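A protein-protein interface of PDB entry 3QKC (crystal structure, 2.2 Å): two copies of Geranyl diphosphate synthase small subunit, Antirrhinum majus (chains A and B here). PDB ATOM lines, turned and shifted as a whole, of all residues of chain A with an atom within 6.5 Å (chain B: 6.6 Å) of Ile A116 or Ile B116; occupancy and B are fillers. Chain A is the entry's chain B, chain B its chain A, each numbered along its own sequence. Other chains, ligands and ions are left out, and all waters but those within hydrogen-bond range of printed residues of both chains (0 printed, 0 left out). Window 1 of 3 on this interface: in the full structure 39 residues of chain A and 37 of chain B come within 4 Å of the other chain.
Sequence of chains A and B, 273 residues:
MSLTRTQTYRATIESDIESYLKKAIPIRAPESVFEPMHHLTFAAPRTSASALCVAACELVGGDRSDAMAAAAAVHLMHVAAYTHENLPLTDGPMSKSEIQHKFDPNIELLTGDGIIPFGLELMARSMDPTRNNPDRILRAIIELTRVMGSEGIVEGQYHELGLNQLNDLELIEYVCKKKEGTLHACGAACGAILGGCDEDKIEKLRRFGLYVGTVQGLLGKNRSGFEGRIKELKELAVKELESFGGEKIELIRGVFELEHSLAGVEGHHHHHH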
ATOM      1  N   ALA A  73     -18.785  -9.188  35.523  1.00  0.00           N
ATOM      2  CA  ALA A  73     -19.569  -9.231  34.291  1.00  0.00           C
ATOM      3  C   ALA A  73     -18.716  -9.763  33.129  1.00  0.00           C
ATOM      4  O   ALA A  73     -19.187 -10.575  32.322  1.00  0.00           O
ATOM      5  CB  ALA A  73     -20.163  -7.850  33.971  1.00  0.00           C
ATOM      6  N   LEU A  76     -18.487 -13.431  33.431  1.00  0.00           N
ATOM      7  CA  LEU A  76     -19.776 -14.017  33.031  1.00  0.00           C
ATOM      8  C   LEU A  76     -20.021 -14.019  31.520  1.00  0.00           C
ATOM      9  O   LEU A  76     -20.547 -15.009  30.979  1.00  0.00           O
ATOM     10  CB  LEU A  76     -20.942 -13.332  33.773  1.00  0.00           C
ATOM     11  CG  LEU A  76     -21.024 -13.644  35.295  1.00  0.00           C
ATOM     12  CD1 LEU A  76     -21.844 -12.585  36.014  1.00  0.00           C
ATOM     13  CD2 LEU A  76     -21.600 -15.037  35.589  1.00  0.00           C
ATOM     14  N   MET A  77     -19.632 -12.948  30.817  1.00  0.00           N
ATOM     15  CA  MET A  77     -19.792 -12.959  29.353  1.00  0.00           C
ATOM     16  C   MET A  77     -19.011 -14.133  28.814  1.00  0.00           C
ATOM     17  O   MET A  77     -19.499 -14.871  27.958  1.00  0.00           O
ATOM     18  CB  MET A  77     -19.307 -11.667  28.667  1.00  0.00           C
ATOM     19  CG  MET A  77     -20.092 -10.402  28.990  1.00  0.00           C
ATOM     20  SD  MET A  77     -21.880 -10.475  28.747  1.00  0.00           S
ATOM     21  CE  MET A  77     -22.346 -10.721  30.479  1.00  0.00           C
ATOM     22  N   ALA A  80     -20.710 -17.337  29.568  1.00  0.00           N
ATOM     23  CA  ALA A  80     -21.821 -17.542  28.646  1.00  0.00           C
ATOM     24  C   ALA A  80     -21.340 -18.037  27.265  1.00  0.00           C
ATOM     25  O   ALA A  80     -21.871 -19.022  26.741  1.00  0.00           O
ATOM     26  CB  ALA A  80     -22.711 -16.314  28.540  1.00  0.00           C
ATOM     27  N   ALA A  81     -20.338 -17.371  26.703  1.00  0.00           N
ATOM     28  CA  ALA A  81     -19.699 -17.800  25.445  1.00  0.00           C
ATOM     29  C   ALA A  81     -19.153 -19.243  25.515  1.00  0.00           C
ATOM     30  O   ALA A  81     -19.444 -20.071  24.636  1.00  0.00           O
ATOM     31  CB  ALA A  81     -18.567 -16.832  25.089  1.00  0.00           C
ATOM     32  N   HIS A  84     -21.965 -21.865  25.638  1.00  0.00           N
ATOM     33  CA  HIS A  84     -22.632 -22.027  24.352  1.00  0.00           C
ATOM     34  C   HIS A  84     -21.761 -22.651  23.267  1.00  0.00           C
ATOM     35  O   HIS A  84     -22.275 -23.356  22.404  1.00  0.00           O
ATOM     36  CB  HIS A  84     -23.250 -20.717  23.905  1.00  0.00           C
ATOM     37  CG  HIS A  84     -24.555 -20.431  24.568  1.00  0.00           C
ATOM     38  ND1 HIS A  84     -25.357 -19.377  24.208  1.00  0.00           N
ATOM     39  CD2 HIS A  84     -25.218 -21.091  25.548  1.00  0.00           C
ATOM     40  CE1 HIS A  84     -26.453 -19.384  24.945  1.00  0.00           C
ATOM     41  NE2 HIS A  84     -26.392 -20.412  25.770  1.00  0.00           N
ATOM     42  N   THR A 111     -29.250 -21.535  30.651  1.00  0.00           N
ATOM     43  CA  THR A 111     -28.367 -20.958  31.666  1.00  0.00           C
ATOM     44  C   THR A 111     -27.427 -19.940  31.038  1.00  0.00           C
ATOM     45  O   THR A 111     -27.126 -18.910  31.655  1.00  0.00           O
ATOM     46  CB  THR A 111     -27.503 -22.015  32.404  1.00  0.00           C
ATOM     47  OG1 THR A 111     -28.341 -23.024  32.959  1.00  0.00           O
ATOM     48  CG2 THR A 111     -26.739 -21.350  33.535  1.00  0.00           C
ATOM     49  N   GLY A 112     -26.939 -20.243  29.834  1.00  0.00           N
ATOM     50  CA  GLY A 112     -26.100 -19.292  29.100  1.00  0.00           C
ATOM     51  C   GLY A 112     -26.902 -18.035  28.830  1.00  0.00           C
ATOM     52  O   GLY A 112     -26.399 -16.928  28.989  1.00  0.00           O
ATOM     53  N   ASP A 113     -28.165 -18.215  28.431  1.00  0.00           N
ATOM     54  CA  ASP A 113     -29.059 -17.085  28.192  1.00  0.00           C
ATOM     55  C   ASP A 113     -29.334 -16.239  29.407  1.00  0.00           C
ATOM     56  O   ASP A 113     -29.451 -15.004  29.288  1.00  0.00           O
ATOM     57  CB  ASP A 113     -30.350 -17.560  27.541  1.00  0.00           C
ATOM     58  CG  ASP A 113     -30.134 -17.935  26.105  1.00  0.00           C
ATOM     59  OD1 ASP A 113     -28.974 -17.799  25.634  1.00  0.00           O
ATOM     60  OD2 ASP A 113     -31.103 -18.345  25.452  1.00  0.00           O
ATOM     61  N   GLY A 114     -29.408 -16.881  30.584  1.00  0.00           N
ATOM     62  CA  GLY A 114     -29.584 -16.116  31.812  1.00  0.00           C
ATOM     63  C   GLY A 114     -28.330 -15.412  32.294  1.00  0.00           C
ATOM     64  O   GLY A 114     -28.408 -14.332  32.865  1.00  0.00           O
ATOM     65  N   ILE A 115     -27.170 -16.035  32.095  1.00  0.00           N
ATOM     66  CA  ILE A 115     -25.886 -15.455  32.500  1.00  0.00           C
ATOM     67  C   ILE A 115     -25.534 -14.153  31.748  1.00  0.00           C
ATOM     68  O   ILE A 115     -24.964 -13.225  32.332  1.00  0.00           O
ATOM     69  CB  ILE A 115     -24.751 -16.482  32.390  1.00  0.00           C
ATOM     70  CG1 ILE A 115     -24.684 -17.403  33.646  1.00  0.00           C
ATOM     71  CG2 ILE A 115     -23.428 -15.823  32.217  1.00  0.00           C
ATOM     72  CD1 ILE A 115     -23.979 -18.716  33.347  1.00  0.00           C
ATOM     73  N   ILE A 116     -25.868 -14.075  30.460  1.00  0.00           N
ATOM     74  CA  ILE A 116     -25.577 -12.847  29.710  1.00  0.00           C
ATOM     75  C   ILE A 116     -26.109 -11.559  30.344  1.00  0.00           C
ATOM     76  O   ILE A 116     -25.315 -10.677  30.605  1.00  0.00           O
ATOM     77  CB  ILE A 116     -25.921 -12.939  28.215  1.00  0.00           C
ATOM     78  CG1 ILE A 116     -24.996 -13.963  27.547  1.00  0.00           C
ATOM     79  CG2 ILE A 116     -25.710 -11.561  27.537  1.00  0.00           C
ATOM     80  CD1 ILE A 116     -25.477 -14.481  26.191  1.00  0.00           C
ATOM     81  N   PRO A 117     -27.428 -11.440  30.598  1.00  0.00           N
ATOM     82  CA  PRO A 117     -27.936 -10.198  31.191  1.00  0.00           C
ATOM     83  C   PRO A 117     -27.623 -10.032  32.698  1.00  0.00           C
ATOM     84  O   PRO A 117     -27.546  -8.900  33.211  1.00  0.00           O
ATOM     85  CB  PRO A 117     -29.455 -10.316  30.996  1.00  0.00           C
ATOM     86  CG  PRO A 117     -29.719 -11.799  30.952  1.00  0.00           C
ATOM     87  CD  PRO A 117     -28.529 -12.332  30.192  1.00  0.00           C
ATOM     88  N   PHE A 118     -27.479 -11.148  33.395  1.00  0.00           N
ATOM     89  CA  PHE A 118     -27.154 -11.150  34.803  1.00  0.00           C
ATOM     90  C   PHE A 118     -25.904 -10.309  35.066  1.00  0.00           C
ATOM     91  O   PHE A 118     -25.898  -9.449  35.941  1.00  0.00           O
ATOM     92  CB  PHE A 118     -26.944 -12.583  35.277  1.00  0.00           C
ATOM     93  CG  PHE A 118     -26.825 -12.714  36.770  1.00  0.00           C
ATOM     94  CD1 PHE A 118     -25.589 -12.628  37.385  1.00  0.00           C
ATOM     95  CD2 PHE A 118     -27.960 -12.914  37.556  1.00  0.00           C
ATOM     96  CE1 PHE A 118     -25.473 -12.743  38.753  1.00  0.00           C
ATOM     97  CE2 PHE A 118     -27.854 -13.032  38.938  1.00  0.00           C
ATOM     98  CZ  PHE A 118     -26.599 -12.946  39.532  1.00  0.00           C
ATOM     99  N   GLY A 119     -24.846 -10.545  34.296  1.00  0.00           N
ATOM    100  CA  GLY A 119     -23.652  -9.711  34.390  1.00  0.00           C
ATOM    101  C   GLY A 119     -23.927  -8.233  34.176  1.00  0.00           C
ATOM    102  O   GLY A 119     -23.407  -7.378  34.918  1.00  0.00           O
ATOM    103  N   LEU A 120     -24.748  -7.920  33.175  1.00  0.00           N
ATOM    104  CA  LEU A 120     -25.136  -6.515  32.912  1.00  0.00           C
ATOM    105  C   LEU A 120     -26.038  -5.935  33.983  1.00  0.00           C
ATOM    106  O   LEU A 120     -25.996  -4.734  34.244  1.00  0.00           O
ATOM    107  CB  LEU A 120     -25.805  -6.358  31.544  1.00  0.00           C
ATOM    108  CG  LEU A 120     -25.000  -6.908  30.362  1.00  0.00           C
ATOM    109  CD1 LEU A 120     -25.903  -7.069  29.162  1.00  0.00           C
ATOM    110  CD2 LEU A 120     -23.845  -5.986  30.057  1.00  0.00           C
ATOM    111  N   GLU A 121     -26.854  -6.791  34.590  1.00  0.00           N
ATOM    112  CA  GLU A 121     -27.680  -6.408  35.746  1.00  0.00           C
ATOM    113  C   GLU A 121     -26.811  -6.091  36.976  1.00  0.00           C
ATOM    114  O   GLU A 121     -27.042  -5.083  37.640  1.00  0.00           O
ATOM    115  CB  GLU A 121     -28.695  -7.501  36.091  1.00  0.00           C
ATOM    116  CG  GLU A 121     -29.673  -7.108  37.198  1.00  0.00           C
ATOM    117  CD  GLU A 121     -30.592  -8.238  37.649  1.00  0.00           C
ATOM    118  OE1 GLU A 121     -30.732  -9.261  36.937  1.00  0.00           O
ATOM    119  OE2 GLU A 121     -31.185  -8.107  38.735  1.00  0.00           O
ATOM    120  N   MET A 148     -20.036  -8.895  23.808  1.00  0.00           N
ATOM    121  CA  MET A 148     -20.810 -10.126  23.715  1.00  0.00           C
ATOM    122  C   MET A 148     -21.312 -10.324  22.287  1.00  0.00           C
ATOM    123  O   MET A 148     -21.417 -11.453  21.826  1.00  0.00           O
ATOM    124  CB  MET A 148     -21.954 -10.091  24.738  1.00  0.00           C
ATOM    125  CG  MET A 148     -22.670 -11.417  25.029  1.00  0.00           C
ATOM    126  SD  MET A 148     -21.647 -12.791  25.677  1.00  0.00           S
ATOM    127  CE  MET A 148     -21.487 -13.697  24.091  1.00  0.00           C
ATOM    128  N   ALA B  73     -35.894  -3.074  22.225  1.00  0.00           N
ATOM    129  CA  ALA B  73     -35.150  -3.991  23.093  1.00  0.00           C
ATOM    130  C   ALA B  73     -36.055  -5.117  23.640  1.00  0.00           C
ATOM    131  O   ALA B  73     -35.643  -6.263  23.738  1.00  0.00           O
ATOM    132  CB  ALA B  73     -34.473  -3.239  24.208  1.00  0.00           C
ATOM    133  N   LEU B  76     -36.582  -7.503  20.801  1.00  0.00           N
ATOM    134  CA  LEU B  76     -35.350  -8.292  20.712  1.00  0.00           C
ATOM    135  C   LEU B  76     -35.197  -9.332  21.829  1.00  0.00           C
ATOM    136  O   LEU B  76     -34.804 -10.456  21.537  1.00  0.00           O
ATOM    137  CB  LEU B  76     -34.104  -7.393  20.615  1.00  0.00           C
ATOM    138  CG  LEU B  76     -34.047  -6.574  19.311  1.00  0.00           C
ATOM    139  CD1 LEU B  76     -33.008  -5.467  19.435  1.00  0.00           C
ATOM    140  CD2 LEU B  76     -33.780  -7.430  18.094  1.00  0.00           C
ATOM    141  N   MET B  77     -35.526  -8.998  23.082  1.00  0.00           N
ATOM    142  CA  MET B  77     -35.478 -10.045  24.134  1.00  0.00           C
ATOM    143  C   MET B  77     -36.403 -11.189  23.727  1.00  0.00           C
ATOM    144  O   MET B  77     -36.021 -12.372  23.780  1.00  0.00           O
ATOM    145  CB  MET B  77     -35.863  -9.540  25.546  1.00  0.00           C
ATOM    146  CG  MET B  77     -34.920  -8.539  26.209  1.00  0.00           C
ATOM    147  SD  MET B  77     -33.155  -8.938  26.200  1.00  0.00           S
ATOM    148  CE  MET B  77     -32.675  -7.956  24.757  1.00  0.00           C
ATOM    149  N   ALA B  80     -34.733 -13.290  20.848  1.00  0.00           N
ATOM    150  CA  ALA B  80     -33.675 -14.166  21.321  1.00  0.00           C
ATOM    151  C   ALA B  80     -34.290 -15.410  21.998  1.00  0.00           C
ATOM    152  O   ALA B  80     -33.925 -16.549  21.666  1.00  0.00           O
ATOM    153  CB  ALA B  80     -32.715 -13.424  22.245  1.00  0.00           C
ATOM    154  N   ALA B  81     -35.259 -15.184  22.882  1.00  0.00           N
ATOM    155  CA  ALA B  81     -35.980 -16.260  23.565  1.00  0.00           C
ATOM    156  C   ALA B  81     -36.654 -17.230  22.576  1.00  0.00           C
ATOM    157  O   ALA B  81     -36.457 -18.443  22.656  1.00  0.00           O
ATOM    158  CB  ALA B  81     -37.015 -15.674  24.518  1.00  0.00           C
ATOM    159  N   HIS B  84     -34.090 -19.334  20.669  1.00  0.00           N
ATOM    160  CA  HIS B  84     -33.513 -20.385  21.476  1.00  0.00           C
ATOM    161  C   HIS B  84     -34.462 -21.510  21.844  1.00  0.00           C
ATOM    162  O   HIS B  84     -34.042 -22.667  21.886  1.00  0.00           O
ATOM    163  CB  HIS B  84     -32.780 -19.846  22.692  1.00  0.00           C
ATOM    164  CG  HIS B  84     -31.448 -19.273  22.355  1.00  0.00           C
ATOM    165  ND1 HIS B  84     -30.692 -18.556  23.252  1.00  0.00           N
ATOM    166  CD2 HIS B  84     -30.738 -19.308  21.203  1.00  0.00           C
ATOM    167  CE1 HIS B  84     -29.565 -18.183  22.671  1.00  0.00           C
ATOM    168  NE2 HIS B  84     -29.572 -18.629  21.428  1.00  0.00           N
ATOM    169  N   THR B 111     -26.710 -16.166  16.914  1.00  0.00           N
ATOM    170  CA  THR B 111     -27.537 -15.001  16.608  1.00  0.00           C
ATOM    171  C   THR B 111     -28.397 -14.644  17.823  1.00  0.00           C
ATOM    172  O   THR B 111     -28.579 -13.465  18.141  1.00  0.00           O
ATOM    173  CB  THR B 111     -28.414 -15.263  15.368  1.00  0.00           C
ATOM    174  OG1 THR B 111     -27.565 -15.637  14.286  1.00  0.00           O
ATOM    175  CG2 THR B 111     -29.185 -14.030  14.970  1.00  0.00           C
ATOM    176  N   GLY B 112     -28.916 -15.669  18.494  1.00  0.00           N
ATOM    177  CA  GLY B 112     -29.677 -15.441  19.731  1.00  0.00           C
ATOM    178  C   GLY B 112     -28.804 -14.738  20.755  1.00  0.00           C
ATOM    179  O   GLY B 112     -29.237 -13.803  21.369  1.00  0.00           O
ATOM    180  N   ASP B 113     -27.553 -15.193  20.907  1.00  0.00           N
ATOM    181  CA  ASP B 113     -26.625 -14.618  21.875  1.00  0.00           C
ATOM    182  C   ASP B 113     -26.223 -13.204  21.547  1.00  0.00           C
ATOM    183  O   ASP B 113     -25.959 -12.418  22.459  1.00  0.00           O
ATOM    184  CB  ASP B 113     -25.387 -15.494  22.048  1.00  0.00           C
ATOM    185  CG  ASP B 113     -25.710 -16.790  22.743  1.00  0.00           C
ATOM    186  OD1 ASP B 113     -26.864 -16.940  23.209  1.00  0.00           O
ATOM    187  OD2 ASP B 113     -24.830 -17.654  22.834  1.00  0.00           O
ATOM    188  N   GLY B 114     -26.148 -12.891  20.247  1.00  0.00           N
ATOM    189  CA  GLY B 114     -25.841 -11.524  19.807  1.00  0.00           C
ATOM    190  C   GLY B 114     -27.007 -10.592  20.019  1.00  0.00           C
ATOM    191  O   GLY B 114     -26.828  -9.453  20.430  1.00  0.00           O
ATOM    192  N   ILE B 115     -28.216 -11.066  19.730  1.00  0.00           N
ATOM    193  CA  ILE B 115     -29.430 -10.261  19.935  1.00  0.00           C
ATOM    194  C   ILE B 115     -29.688  -9.812  21.398  1.00  0.00           C
ATOM    195  O   ILE B 115     -30.188  -8.690  21.647  1.00  0.00           O
ATOM    196  CB  ILE B 115     -30.668 -10.980  19.366  1.00  0.00           C
ATOM    197  CG1 ILE B 115     -30.743 -10.785  17.832  1.00  0.00           C
ATOM    198  CG2 ILE B 115     -31.932 -10.438  20.002  1.00  0.00           C
ATOM    199  CD1 ILE B 115     -31.517 -11.887  17.080  1.00  0.00           C
ATOM    200  N   ILE B 116     -29.357 -10.656  22.369  1.00  0.00           N
ATOM    201  CA  ILE B 116     -29.592 -10.276  23.767  1.00  0.00           C
ATOM    202  C   ILE B 116     -28.928  -8.959  24.167  1.00  0.00           C
ATOM    203  O   ILE B 116     -29.622  -8.055  24.586  1.00  0.00           O
ATOM    204  CB  ILE B 116     -29.295 -11.420  24.782  1.00  0.00           C
ATOM    205  CG1 ILE B 116     -30.298 -12.563  24.572  1.00  0.00           C
ATOM    206  CG2 ILE B 116     -29.405 -10.893  26.205  1.00  0.00           C
ATOM    207  CD1 ILE B 116     -30.006 -13.818  25.411  1.00  0.00           C
ATOM    208  N   PRO B 117     -27.590  -8.837  24.034  1.00  0.00           N
ATOM    209  CA  PRO B 117     -26.952  -7.580  24.410  1.00  0.00           C
ATOM    210  C   PRO B 117     -27.234  -6.399  23.446  1.00  0.00           C
ATOM    211  O   PRO B 117     -27.147  -5.222  23.851  1.00  0.00           O
ATOM    212  CB  PRO B 117     -25.458  -7.929  24.403  1.00  0.00           C
ATOM    213  CG  PRO B 117     -25.336  -9.040  23.420  1.00  0.00           C
ATOM    214  CD  PRO B 117     -26.606  -9.845  23.601  1.00  0.00           C
ATOM    215  N   PHE B 118     -27.558  -6.712  22.192  1.00  0.00           N
ATOM    216  CA  PHE B 118     -27.820  -5.700  21.172  1.00  0.00           C
ATOM    217  C   PHE B 118     -28.950  -4.745  21.604  1.00  0.00           C
ATOM    218  O   PHE B 118     -28.813  -3.524  21.523  1.00  0.00           O
ATOM    219  CB  PHE B 118     -28.143  -6.387  19.845  1.00  0.00           C
ATOM    220  CG  PHE B 118     -28.095  -5.469  18.651  1.00  0.00           C
ATOM    221  CD1 PHE B 118     -29.218  -4.742  18.273  1.00  0.00           C
ATOM    222  CD2 PHE B 118     -26.914  -5.326  17.913  1.00  0.00           C
ATOM    223  CE1 PHE B 118     -29.183  -3.891  17.183  1.00  0.00           C
ATOM    224  CE2 PHE B 118     -26.856  -4.462  16.803  1.00  0.00           C
ATOM    225  CZ  PHE B 118     -27.995  -3.741  16.437  1.00  0.00           C
ATOM    226  N   GLY B 119     -30.059  -5.316  22.079  1.00  0.00           N
ATOM    227  CA  GLY B 119     -31.173  -4.534  22.609  1.00  0.00           C
ATOM    228  C   GLY B 119     -30.771  -3.639  23.780  1.00  0.00           C
ATOM    229  O   GLY B 119     -31.180  -2.455  23.853  1.00  0.00           O
ATOM    230  N   LEU B 120     -29.956  -4.191  24.682  1.00  0.00           N
ATOM    231  CA  LEU B 120     -29.449  -3.432  25.832  1.00  0.00           C
ATOM    232  C   LEU B 120     -28.503  -2.343  25.375  1.00  0.00           C
ATOM    233  O   LEU B 120     -28.498  -1.257  25.944  1.00  0.00           O
ATOM    234  CB  LEU B 120     -28.772  -4.337  26.875  1.00  0.00           C
ATOM    235  CG  LEU B 120     -29.666  -5.491  27.362  1.00  0.00           C
ATOM    236  CD1 LEU B 120     -28.844  -6.553  28.060  1.00  0.00           C
ATOM    237  CD2 LEU B 120     -30.764  -5.001  28.271  1.00  0.00           C
ATOM    238  N   GLU B 121     -27.736  -2.636  24.330  1.00  0.00           N
ATOM    239  CA  GLU B 121     -26.865  -1.639  23.692  1.00  0.00           C
ATOM    240  C   GLU B 121     -27.666  -0.532  23.004  1.00  0.00           C
ATOM    241  O   GLU B 121     -27.317   0.651  23.143  1.00  0.00           O
ATOM    242  CB  GLU B 121     -25.896  -2.278  22.697  1.00  0.00           C
ATOM    243  CG  GLU B 121     -24.899  -1.290  22.113  1.00  0.00           C
ATOM    244  CD  GLU B 121     -24.006  -1.874  21.025  1.00  0.00           C
ATOM    245  OE1 GLU B 121     -24.056  -3.104  20.752  1.00  0.00           O
ATOM    246  OE2 GLU B 121     -23.234  -1.086  20.445  1.00  0.00           O
ATOM    247  N   MET B 148     -35.053 -11.053  30.986  1.00  0.00           N
ATOM    248  CA  MET B 148     -34.371 -12.076  30.217  1.00  0.00           C
ATOM    249  C   MET B 148     -33.906 -13.192  31.135  1.00  0.00           C
ATOM    250  O   MET B 148     -33.886 -14.343  30.726  1.00  0.00           O
ATOM    251  CB  MET B 148     -33.197 -11.426  29.463  1.00  0.00           C
ATOM    252  CG  MET B 148     -32.586 -12.234  28.337  1.00  0.00           C
ATOM    253  SD  MET B 148     -33.679 -12.647  26.934  1.00  0.00           S
ATOM    254  CE  MET B 148     -33.883 -14.421  27.365  1.00  0.00           C
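OD1 of Asp B113 lies close to ND1 of His A84 (3.0 Å).
ND1 of His B84 sits close to OD1 of Asp A113, at 3.0 Å.
The side-chain carboxylate (OD1) of Asp A113 sits close to the side-chain carboxylate (OD1) of Asp B113 (3.3 Å).
Of the printed residues of chain B, Ile A116 touches Ile B116.
Of the printed residues of chain A, Ile B116 touches Ile A116 (3.98 Å).
Of the printed residues of chain A, Met B148 touches Pro A117.
Of the printed residues of chain A, His B84 touches Asp A113 (2.2 Å).
Of the printed residues of chain B, Leu A120 touches Leu B120.
Ile A115 touches none of the printed residues of chain B.
Of the 18 printed residues of chain A, 6 touch a printed residue of chain B.
Hydrophobic or aromatic side chains of chain A that line the printed part of chain B: His A84, Ile A116, Pro A117, Leu A120 and Met A148.
Of the 18 printed residues of chain B, 6 touch a printed residue of chain A.
Hydrophobic or aromatic side chains of chain B within 4 Å of the printed part of chain A: His B84, Ile B116, Pro B117, Leu B120 and Met B148.
Along chain B the printed residues that touch a printed residue of chain A span positions 84 to 148.
Among the printed residues, 7 pairs touch across the chains.
Among the printed residues, pairs that only touch across the chains: Leu A120 with Leu B120 (3.2 Å), Met A148 with Pro B117 (3.8 Å), Pro A117 with Met B148 (3.8 Å) and Ile A116 with Ile B116 (3.98 Å).
His A84 touches Asp B113, and with the chains exchanged Asp A113 touches His B84.
Asp B113 touches its own counterpart, Asp A113.
Ile B116 touches its own counterpart, Ile A116.
Pro A117 touches Met B148, and with the chains exchanged Met A148 touches Pro B117.
Positions printed for both chains: 73, 76, 77, 80, 81, 84, 111, 112, 113, 114, 115, 116, 117, 118, 119, 120, 121 and 148.
Of the 7 pairs that touch across the chains among the printed residues, 7 have their exchanged pair printed and touching as well.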
